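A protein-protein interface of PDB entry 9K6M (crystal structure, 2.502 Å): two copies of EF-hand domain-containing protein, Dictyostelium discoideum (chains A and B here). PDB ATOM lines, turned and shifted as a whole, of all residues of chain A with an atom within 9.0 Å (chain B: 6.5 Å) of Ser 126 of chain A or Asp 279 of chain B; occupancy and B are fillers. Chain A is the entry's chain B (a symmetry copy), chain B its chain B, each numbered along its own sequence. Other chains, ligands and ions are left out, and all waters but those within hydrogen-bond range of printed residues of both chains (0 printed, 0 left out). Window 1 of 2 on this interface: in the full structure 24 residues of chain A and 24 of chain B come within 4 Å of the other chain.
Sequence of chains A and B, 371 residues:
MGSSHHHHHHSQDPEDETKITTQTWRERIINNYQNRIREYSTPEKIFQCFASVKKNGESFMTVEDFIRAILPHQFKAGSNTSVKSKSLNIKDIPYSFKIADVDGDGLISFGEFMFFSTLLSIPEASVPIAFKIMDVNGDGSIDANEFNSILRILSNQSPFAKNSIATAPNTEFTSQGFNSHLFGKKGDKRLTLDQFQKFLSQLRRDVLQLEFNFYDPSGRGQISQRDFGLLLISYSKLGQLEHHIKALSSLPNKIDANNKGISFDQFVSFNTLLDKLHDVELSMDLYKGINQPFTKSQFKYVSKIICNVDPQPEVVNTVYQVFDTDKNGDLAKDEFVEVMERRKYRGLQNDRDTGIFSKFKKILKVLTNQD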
ATOM      1  N   SER A 121      17.383  26.815 -11.274  1.00  0.00           N
ATOM      2  CA  SER A 121      17.742  26.553 -12.660  1.00  0.00           C
ATOM      3  C   SER A 121      18.814  25.461 -12.742  1.00  0.00           C
ATOM      4  O   SER A 121      19.002  24.881 -13.812  1.00  0.00           O
ATOM      5  CB  SER A 121      18.165  27.812 -13.404  1.00  0.00           C
ATOM      6  OG  SER A 121      19.502  28.160 -13.090  1.00  0.00           O
ATOM      7  N   ILE A 122      19.508  25.162 -11.633  1.00  0.00           N
ATOM      8  CA  ILE A 122      20.638  24.247 -11.704  1.00  0.00           C
ATOM      9  C   ILE A 122      20.114  22.831 -11.943  1.00  0.00           C
ATOM     10  O   ILE A 122      19.311  22.311 -11.171  1.00  0.00           O
ATOM     11  CB  ILE A 122      21.541  24.329 -10.463  1.00  0.00           C
ATOM     12  CG1 ILE A 122      22.109  25.733 -10.251  1.00  0.00           C
ATOM     13  CG2 ILE A 122      22.661  23.307 -10.565  1.00  0.00           C
ATOM     14  CD1 ILE A 122      22.682  25.964  -8.875  1.00  0.00           C
ATOM     15  N   PRO A 123      20.508  22.176 -13.048  1.00  0.00           N
ATOM     16  CA  PRO A 123      20.144  20.775 -13.300  1.00  0.00           C
ATOM     17  C   PRO A 123      20.827  19.787 -12.361  1.00  0.00           C
ATOM     18  O   PRO A 123      21.996  19.953 -12.038  1.00  0.00           O
ATOM     19  CB  PRO A 123      20.617  20.536 -14.743  1.00  0.00           C
ATOM     20  CG  PRO A 123      20.788  21.943 -15.318  1.00  0.00           C
ATOM     21  CD  PRO A 123      21.287  22.761 -14.145  1.00  0.00           C
ATOM     22  N   GLU A 124      20.100  18.758 -11.927  1.00  0.00           N
ATOM     23  CA  GLU A 124      20.584  17.864 -10.888  1.00  0.00           C
ATOM     24  C   GLU A 124      21.966  17.312 -11.225  1.00  0.00           C
ATOM     25  O   GLU A 124      22.790  17.116 -10.327  1.00  0.00           O
ATOM     26  CB  GLU A 124      19.609  16.706 -10.685  1.00  0.00           C
ATOM     27  CG  GLU A 124      19.940  15.848  -9.469  1.00  0.00           C
ATOM     28  CD  GLU A 124      19.131  14.569  -9.302  1.00  0.00           C
ATOM     29  OE1 GLU A 124      18.365  14.202 -10.223  1.00  0.00           O
ATOM     30  OE2 GLU A 124      19.259  13.939  -8.227  1.00  0.00           O
ATOM     31  N   ALA A 125      22.179  17.025 -12.513  1.00  0.00           N
ATOM     32  CA  ALA A 125      23.417  16.419 -12.983  1.00  0.00           C
ATOM     33  C   ALA A 125      24.598  17.391 -12.927  1.00  0.00           C
ATOM     34  O   ALA A 125      25.719  16.918 -12.963  1.00  0.00           O
ATOM     35  CB  ALA A 125      23.219  15.905 -14.392  1.00  0.00           C
ATOM     36  N   SER A 126      24.345  18.708 -12.835  1.00  0.00           N
ATOM     37  CA  SER A 126      25.377  19.734 -12.910  1.00  0.00           C
ATOM     38  C   SER A 126      25.581  20.430 -11.563  1.00  0.00           C
ATOM     39  O   SER A 126      26.302  21.404 -11.464  1.00  0.00           O
ATOM     40  CB  SER A 126      25.005  20.711 -13.973  1.00  0.00           C
ATOM     41  OG  SER A 126      24.684  20.025 -15.181  1.00  0.00           O
ATOM     42  N   VAL A 127      24.952  19.913 -10.511  1.00  0.00           N
ATOM     43  CA  VAL A 127      25.048  20.506  -9.195  1.00  0.00           C
ATOM     44  C   VAL A 127      26.495  20.482  -8.700  1.00  0.00           C
ATOM     45  O   VAL A 127      26.930  21.420  -8.034  1.00  0.00           O
ATOM     46  CB  VAL A 127      24.076  19.804  -8.229  1.00  0.00           C
ATOM     47  CG1 VAL A 127      24.346  20.134  -6.771  1.00  0.00           C
ATOM     48  CG2 VAL A 127      22.646  20.152  -8.577  1.00  0.00           C
ATOM     49  N   PRO A 128      27.283  19.413  -8.957  1.00  0.00           N
ATOM     50  CA  PRO A 128      28.714  19.417  -8.610  1.00  0.00           C
ATOM     51  C   PRO A 128      29.525  20.553  -9.237  1.00  0.00           C
ATOM     52  O   PRO A 128      30.453  21.059  -8.611  1.00  0.00           O
ATOM     53  CB  PRO A 128      29.190  18.032  -9.103  1.00  0.00           C
ATOM     54  CG  PRO A 128      27.942  17.173  -9.039  1.00  0.00           C
ATOM     55  CD  PRO A 128      26.850  18.114  -9.513  1.00  0.00           C
ATOM     56  N   ILE A 129      29.159  20.975 -10.449  1.00  0.00           N
ATOM     57  CA  ILE A 129      29.843  22.065 -11.132  1.00  0.00           C
ATOM     58  C   ILE A 129      29.516  23.374 -10.419  1.00  0.00           C
ATOM     59  O   ILE A 129      30.418  24.153 -10.079  1.00  0.00           O
ATOM     60  CB  ILE A 129      29.488  22.134 -12.635  1.00  0.00           C
ATOM     61  CG1 ILE A 129      29.622  20.768 -13.325  1.00  0.00           C
ATOM     62  CG2 ILE A 129      30.314  23.188 -13.359  1.00  0.00           C
ATOM     63  CD1 ILE A 129      31.039  20.224 -13.406  1.00  0.00           C
ATOM     64  N   ALA A 130      28.211  23.577 -10.193  1.00  0.00           N
ATOM     65  CA  ALA A 130      27.714  24.738  -9.475  1.00  0.00           C
ATOM     66  C   ALA A 130      28.287  24.808  -8.058  1.00  0.00           C
ATOM     67  O   ALA A 130      28.665  25.875  -7.598  1.00  0.00           O
ATOM     68  CB  ALA A 130      26.207  24.722  -9.491  1.00  0.00           C
ATOM     69  N   PHE A 131      28.434  23.657  -7.397  1.00  0.00           N
ATOM     70  CA  PHE A 131      29.039  23.621  -6.071  1.00  0.00           C
ATOM     71  C   PHE A 131      30.467  24.188  -6.087  1.00  0.00           C
ATOM     72  O   PHE A 131      30.853  24.892  -5.169  1.00  0.00           O
ATOM     73  CB  PHE A 131      29.004  22.198  -5.498  1.00  0.00           C
ATOM     74  CG  PHE A 131      29.487  22.093  -4.073  1.00  0.00           C
ATOM     75  CD1 PHE A 131      28.639  22.337  -3.002  1.00  0.00           C
ATOM     76  CD2 PHE A 131      30.812  21.773  -3.803  1.00  0.00           C
ATOM     77  CE1 PHE A 131      29.100  22.238  -1.696  1.00  0.00           C
ATOM     78  CE2 PHE A 131      31.275  21.676  -2.496  1.00  0.00           C
ATOM     79  CZ  PHE A 131      30.419  21.917  -1.443  1.00  0.00           C
ATOM     80  N   LYS A 132      31.253  23.862  -7.116  1.00  0.00           N
ATOM     81  CA  LYS A 132      32.670  24.208  -7.146  1.00  0.00           C
ATOM     82  C   LYS A 132      32.832  25.693  -7.432  1.00  0.00           C
ATOM     83  O   LYS A 132      33.727  26.336  -6.894  1.00  0.00           O
ATOM     84  CB  LYS A 132      33.425  23.344  -8.157  1.00  0.00           C
ATOM     85  CG  LYS A 132      33.697  21.922  -7.682  1.00  0.00           C
ATOM     86  CD  LYS A 132      34.505  21.111  -8.642  1.00  0.00           C
ATOM     87  CE  LYS A 132      34.733  19.694  -8.171  1.00  0.00           C
ATOM     88  NZ  LYS A 132      35.401  18.898  -9.234  1.00  0.00           N
ATOM     89  N   ILE A 133      31.935  26.241  -8.233  1.00  0.00           N
ATOM     90  CA  ILE A 133      31.962  27.657  -8.535  1.00  0.00           C
ATOM     91  C   ILE A 133      31.632  28.437  -7.273  1.00  0.00           C
ATOM     92  O   ILE A 133      32.125  29.535  -7.091  1.00  0.00           O
ATOM     93  CB  ILE A 133      30.997  27.947  -9.692  1.00  0.00           C
ATOM     94  CG1 ILE A 133      31.539  27.314 -10.973  1.00  0.00           C
ATOM     95  CG2 ILE A 133      30.750  29.445  -9.824  1.00  0.00           C
ATOM     96  CD1 ILE A 133      30.654  27.504 -12.171  1.00  0.00           C
ATOM     97  N   MET A 134      30.789  27.858  -6.426  1.00  0.00           N
ATOM     98  CA  MET A 134      30.297  28.564  -5.270  1.00  0.00           C
ATOM     99  C   MET A 134      31.264  28.392  -4.114  1.00  0.00           C
ATOM    100  O   MET A 134      31.323  29.286  -3.286  1.00  0.00           O
ATOM    101  CB  MET A 134      28.904  28.079  -4.890  1.00  0.00           C
ATOM    102  CG  MET A 134      27.822  28.777  -5.684  1.00  0.00           C
ATOM    103  SD  MET A 134      26.175  28.163  -5.254  1.00  0.00           S
ATOM    104  CE  MET A 134      25.318  28.571  -6.775  1.00  0.00           C
ATOM    105  N   LEU A 193      28.673  18.928  -0.538  1.00  0.00           N
ATOM    106  CA  LEU A 193      28.053  18.737  -1.839  1.00  0.00           C
ATOM    107  C   LEU A 193      26.799  17.861  -1.733  1.00  0.00           C
ATOM    108  O   LEU A 193      25.826  18.130  -2.427  1.00  0.00           O
ATOM    109  CB  LEU A 193      29.077  18.143  -2.815  1.00  0.00           C
ATOM    110  CG  LEU A 193      28.491  17.552  -4.100  1.00  0.00           C
ATOM    111  CD1 LEU A 193      27.938  18.616  -5.036  1.00  0.00           C
ATOM    112  CD2 LEU A 193      29.537  16.727  -4.815  1.00  0.00           C
ATOM    113  N   PHE A 196      24.075  19.945  -0.319  1.00  0.00           N
ATOM    114  CA  PHE A 196      23.657  20.935  -1.294  1.00  0.00           C
ATOM    115  C   PHE A 196      22.784  20.279  -2.341  1.00  0.00           C
ATOM    116  O   PHE A 196      21.826  20.893  -2.782  1.00  0.00           O
ATOM    117  CB  PHE A 196      24.881  21.558  -1.959  1.00  0.00           C
ATOM    118  CG  PHE A 196      24.668  22.690  -2.939  1.00  0.00           C
ATOM    119  CD1 PHE A 196      24.110  23.898  -2.542  1.00  0.00           C
ATOM    120  CD2 PHE A 196      25.143  22.589  -4.240  1.00  0.00           C
ATOM    121  CE1 PHE A 196      23.985  24.952  -3.435  1.00  0.00           C
ATOM    122  CE2 PHE A 196      25.034  23.651  -5.125  1.00  0.00           C
ATOM    123  CZ  PHE A 196      24.459  24.835  -4.725  1.00  0.00           C
ATOM    124  N   GLN A 197      23.149  19.052  -2.737  1.00  0.00           N
ATOM    125  CA  GLN A 197      22.351  18.270  -3.663  1.00  0.00           C
ATOM    126  C   GLN A 197      20.982  18.025  -3.039  1.00  0.00           C
ATOM    127  O   GLN A 197      19.967  18.242  -3.685  1.00  0.00           O
ATOM    128  CB  GLN A 197      23.051  16.958  -4.021  1.00  0.00           C
ATOM    129  CG  GLN A 197      24.212  17.116  -4.989  1.00  0.00           C
ATOM    130  CD  GLN A 197      24.978  15.823  -5.165  1.00  0.00           C
ATOM    131  OE1 GLN A 197      25.456  15.214  -4.208  1.00  0.00           O
ATOM    132  NE2 GLN A 197      25.110  15.391  -6.408  1.00  0.00           N
ATOM    133  N   LEU A 200      18.804  21.291  -2.976  1.00  0.00           N
ATOM    134  CA  LEU A 200      18.275  21.648  -4.285  1.00  0.00           C
ATOM    135  C   LEU A 200      17.163  20.680  -4.680  1.00  0.00           C
ATOM    136  O   LEU A 200      16.208  21.088  -5.337  1.00  0.00           O
ATOM    137  CB  LEU A 200      19.417  21.697  -5.309  1.00  0.00           C
ATOM    138  CG  LEU A 200      20.471  22.780  -5.068  1.00  0.00           C
ATOM    139  CD1 LEU A 200      21.446  22.854  -6.220  1.00  0.00           C
ATOM    140  CD2 LEU A 200      19.848  24.152  -4.845  1.00  0.00           C
ATOM    141  N   ARG A 204      13.382  21.725  -5.747  1.00  0.00           N
ATOM    142  CA  ARG A 204      12.759  21.350  -7.002  1.00  0.00           C
ATOM    143  C   ARG A 204      11.433  20.636  -6.750  1.00  0.00           C
ATOM    144  O   ARG A 204      10.441  20.973  -7.403  1.00  0.00           O
ATOM    145  CB  ARG A 204      13.746  20.531  -7.823  1.00  0.00           C
ATOM    146  CG  ARG A 204      14.901  21.341  -8.404  1.00  0.00           C
ATOM    147  CD  ARG A 204      15.874  20.559  -9.311  1.00  0.00           C
ATOM    148  NE  ARG A 204      16.421  19.322  -8.744  1.00  0.00           N
ATOM    149  CZ  ARG A 204      17.657  19.152  -8.293  1.00  0.00           C
ATOM    150  NH1 ARG A 204      18.563  20.098  -8.437  1.00  0.00           N
ATOM    151  NH2 ARG A 204      17.979  18.041  -7.654  1.00  0.00           N
ATOM    152  N   TYR A 345      19.594  25.544 -19.792  1.00  0.00           N
ATOM    153  CA  TYR A 345      20.773  24.682 -20.090  1.00  0.00           C
ATOM    154  C   TYR A 345      20.302  23.540 -20.994  1.00  0.00           C
ATOM    155  O   TYR A 345      19.882  23.797 -22.123  1.00  0.00           O
ATOM    156  CB  TYR A 345      21.441  24.356 -18.744  1.00  0.00           C
ATOM    157  CG  TYR A 345      21.571  25.608 -17.885  1.00  0.00           C
ATOM    158  CD1 TYR A 345      22.146  26.760 -18.403  1.00  0.00           C
ATOM    159  CD2 TYR A 345      21.035  25.674 -16.602  1.00  0.00           C
ATOM    160  CE1 TYR A 345      22.224  27.922 -17.658  1.00  0.00           C
ATOM    161  CE2 TYR A 345      21.102  26.832 -15.844  1.00  0.00           C
ATOM    162  CZ  TYR A 345      21.708  27.958 -16.371  1.00  0.00           C
ATOM    163  OH  TYR A 345      21.788  29.108 -15.631  1.00  0.00           O
ATOM    164  N   ARG A 346      20.354  22.288 -20.517  1.00  0.00           N
ATOM    165  CA  ARG A 346      20.031  21.155 -21.375  1.00  0.00           C
ATOM    166  C   ARG A 346      18.522  21.133 -21.642  1.00  0.00           C
ATOM    167  O   ARG A 346      18.151  21.334 -22.814  1.00  0.00           O
ATOM    168  CB  ARG A 346      20.496  19.833 -20.756  1.00  0.00           C
ATOM    169  N   LYS B 276      30.040  19.032 -23.055  1.00  0.00           N
ATOM    170  CA  LYS B 276      29.396  19.512 -21.842  1.00  0.00           C
ATOM    171  C   LYS B 276      29.138  21.012 -21.927  1.00  0.00           C
ATOM    172  O   LYS B 276      29.343  21.736 -20.962  1.00  0.00           O
ATOM    173  CB  LYS B 276      30.286  19.219 -20.640  1.00  0.00           C
ATOM    174  CG  LYS B 276      30.688  17.765 -20.495  1.00  0.00           C
ATOM    175  CD  LYS B 276      29.682  16.941 -19.721  1.00  0.00           C
ATOM    176  CE  LYS B 276      30.295  15.701 -19.102  1.00  0.00           C
ATOM    177  NZ  LYS B 276      31.377  16.048 -18.147  1.00  0.00           N
ATOM    178  N   LEU B 277      28.665  21.471 -23.082  1.00  0.00           N
ATOM    179  CA  LEU B 277      28.509  22.887 -23.352  1.00  0.00           C
ATOM    180  C   LEU B 277      27.386  23.491 -22.506  1.00  0.00           C
ATOM    181  O   LEU B 277      27.308  24.706 -22.314  1.00  0.00           O
ATOM    182  CB  LEU B 277      28.201  22.993 -24.844  1.00  0.00           C
ATOM    183  CG  LEU B 277      28.693  24.256 -25.531  1.00  0.00           C
ATOM    184  CD1 LEU B 277      30.211  24.338 -25.484  1.00  0.00           C
ATOM    185  CD2 LEU B 277      28.199  24.290 -26.973  1.00  0.00           C
ATOM    186  N   HIS B 278      26.478  22.631 -22.034  1.00  0.00           N
ATOM    187  CA  HIS B 278      25.414  23.045 -21.137  1.00  0.00           C
ATOM    188  C   HIS B 278      26.038  23.486 -19.816  1.00  0.00           C
ATOM    189  O   HIS B 278      25.583  24.429 -19.186  1.00  0.00           O
ATOM    190  CB  HIS B 278      24.389  21.909 -20.975  1.00  0.00           C
ATOM    191  CG  HIS B 278      24.971  20.558 -20.650  1.00  0.00           C
ATOM    192  ND1 HIS B 278      25.434  19.681 -21.612  1.00  0.00           N
ATOM    193  CD2 HIS B 278      25.135  19.928 -19.468  1.00  0.00           C
ATOM    194  CE1 HIS B 278      25.883  18.573 -21.026  1.00  0.00           C
ATOM    195  NE2 HIS B 278      25.717  18.703 -19.722  1.00  0.00           N
ATOM    196  N   ASP B 279      27.085  22.762 -19.398  1.00  0.00           N
ATOM    197  CA  ASP B 279      27.743  22.989 -18.124  1.00  0.00           C
ATOM    198  C   ASP B 279      28.517  24.301 -18.195  1.00  0.00           C
ATOM    199  O   ASP B 279      28.624  24.992 -17.183  1.00  0.00           O
ATOM    200  CB  ASP B 279      28.580  21.775 -17.714  1.00  0.00           C
ATOM    201  CG  ASP B 279      27.778  20.733 -16.944  1.00  0.00           C
ATOM    202  OD1 ASP B 279      26.670  21.067 -16.516  1.00  0.00           O
ATOM    203  OD2 ASP B 279      28.258  19.579 -16.791  1.00  0.00           O
ATOM    204  N   VAL B 280      29.008  24.651 -19.396  1.00  0.00           N
ATOM    205  CA  VAL B 280      29.689  25.922 -19.604  1.00  0.00           C
ATOM    206  C   VAL B 280      28.656  27.048 -19.468  1.00  0.00           C
ATOM    207  O   VAL B 280      28.902  28.030 -18.775  1.00  0.00           O
ATOM    208  CB  VAL B 280      30.454  25.957 -20.947  1.00  0.00           C
ATOM    209  CG1 VAL B 280      30.931  27.346 -21.306  1.00  0.00           C
ATOM    210  CG2 VAL B 280      31.633  25.005 -20.948  1.00  0.00           C
ATOM    211  N   GLU B 281      27.482  26.870 -20.091  1.00  0.00           N
ATOM    212  CA  GLU B 281      26.403  27.840 -20.012  1.00  0.00           C
ATOM    213  C   GLU B 281      25.927  28.047 -18.567  1.00  0.00           C
ATOM    214  O   GLU B 281      25.678  29.179 -18.128  1.00  0.00           O
ATOM    215  CB  GLU B 281      25.256  27.369 -20.897  1.00  0.00           C
ATOM    216  CG  GLU B 281      24.186  28.420 -21.086  1.00  0.00           C
ATOM    217  CD  GLU B 281      22.923  27.954 -21.799  1.00  0.00           C
ATOM    218  OE1 GLU B 281      22.931  26.842 -22.397  1.00  0.00           O
ATOM    219  OE2 GLU B 281      21.927  28.704 -21.734  1.00  0.00           O
ATOM    220  N   LEU B 282      25.764  26.964 -17.806  1.00  0.00           N
ATOM    221  CA  LEU B 282      25.411  27.143 -16.411  1.00  0.00           C
ATOM    222  C   LEU B 282      26.411  28.091 -15.762  1.00  0.00           C
ATOM    223  O   LEU B 282      26.028  29.039 -15.093  1.00  0.00           O
ATOM    224  CB  LEU B 282      25.423  25.790 -15.706  1.00  0.00           C
ATOM    225  CG  LEU B 282      25.246  25.837 -14.192  1.00  0.00           C
ATOM    226  CD1 LEU B 282      23.931  26.502 -13.812  1.00  0.00           C
ATOM    227  CD2 LEU B 282      25.307  24.431 -13.612  1.00  0.00           C
ATOM    228  N   SER B 283      27.699  27.808 -15.957  1.00  0.00           N
ATOM    229  CA  SER B 283      28.755  28.497 -15.238  1.00  0.00           C
ATOM    230  C   SER B 283      28.727  29.989 -15.596  1.00  0.00           C
ATOM    231  O   SER B 283      29.072  30.836 -14.773  1.00  0.00           O
ATOM    232  CB  SER B 283      30.122  27.874 -15.535  1.00  0.00           C
ATOM    233  OG  SER B 283      30.170  26.476 -15.249  1.00  0.00           O
ATOM    234  N   MET B 284      28.346  30.307 -16.846  1.00  0.00           N
ATOM    235  CA  MET B 284      28.310  31.685 -17.297  1.00  0.00           C
ATOM    236  C   MET B 284      27.263  32.455 -16.487  1.00  0.00           C
ATOM    237  O   MET B 284      27.478  33.614 -16.129  1.00  0.00           O
ATOM    238  CB  MET B 284      27.989  31.767 -18.793  1.00  0.00           C
ATOM    239  CG  MET B 284      29.211  31.597 -19.687  1.00  0.00           C
ATOM    240  SD  MET B 284      28.758  31.245 -21.420  1.00  0.00           S
ATOM    241  CE  MET B 284      30.334  31.354 -22.273  1.00  0.00           C
ATOM    242  N   VAL B 302      36.480  26.761 -15.197  1.00  0.00           N
ATOM    243  CA  VAL B 302      35.321  25.967 -15.591  1.00  0.00           C
ATOM    244  C   VAL B 302      35.792  24.775 -16.413  1.00  0.00           C
ATOM    245  O   VAL B 302      35.361  23.641 -16.209  1.00  0.00           O
ATOM    246  CB  VAL B 302      34.318  26.791 -16.419  1.00  0.00           C
ATOM    247  CG1 VAL B 302      33.373  25.929 -17.229  1.00  0.00           C
ATOM    248  CG2 VAL B 302      33.527  27.731 -15.544  1.00  0.00           C
ATOM    249  N   ILE B 306      35.301  20.754 -15.547  1.00  0.00           N
ATOM    250  CA  ILE B 306      34.476  19.957 -16.449  1.00  0.00           C
ATOM    251  C   ILE B 306      35.254  18.814 -17.110  1.00  0.00           C
ATOM    252  O   ILE B 306      34.724  17.706 -17.266  1.00  0.00           O
ATOM    253  CB  ILE B 306      33.855  20.835 -17.538  1.00  0.00           C
ATOM    254  CG1 ILE B 306      32.690  21.649 -16.996  1.00  0.00           C
ATOM    255  CG2 ILE B 306      33.460  19.975 -18.720  1.00  0.00           C
ATOM    256  CD1 ILE B 306      32.131  22.645 -18.012  1.00  0.00           C
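The side-chain carboxylate (OD1) of Asp 279 of chain B sits at hydrogen-bond distance from the side-chain hydroxyl (OG) of Ser 126 of chain A, at 2.6 Å.
OG of Ser 283 of chain B is in hydrogen-bond range of O of Asp 279 of chain B (2.9 Å).
Among the printed residues, merely in contact across the chains: Ser 126 of chain A with Leu 282 of chain B, Ile 129 of chain A with Asp 279 of chain B, Ile 129 of chain A with Ser 283 of chain B, Ile 133 of chain A with Ser 283 of chain B, Tyr 345 of chain A with Glu 281 of chain B and Tyr 345 of chain A with Leu 282 of chain B.
Printed residues of chain B within 4 Å of Ser 126 of chain A: Asp 279 and Leu 282. Of the printed residues of chain A, Asp 279 of chain B touches Ser 126 and Ile 129. No residue of chain A comes within 4 Å of His 278 of chain B. Of the printed residues of chain A, Ser 283 of chain B touches Ile 129 and Ile 133. Printed residues of chain A within 4 Å of Leu 282 of chain B: Ser 126 (3.7 Å) and Tyr 345 (3.5 Å). Phe 131 of chain A touches none of the printed residues of chain B. The nearest printed residue of chain A that does not touch Ser 283 of chain B is Tyr 345 of chain A (5.7 Å).
Of the 11 printed residues of chain B, 4 touch a printed residue of chain A. Hydrophobic or aromatic side chains of chain B within 4 Å of the printed part of chain A: Leu 282. Among the printed residues, 7 pairs touch across the chains. Among the printed residues, no Asp or Glu carboxylate lies within 4 Å of a Lys or Arg side-chain nitrogen of the other chain.
No position is printed for both chains. Of the 7 pairs that touch across the chains among the printed residues, none has its exchanged pair printed and touching as well.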
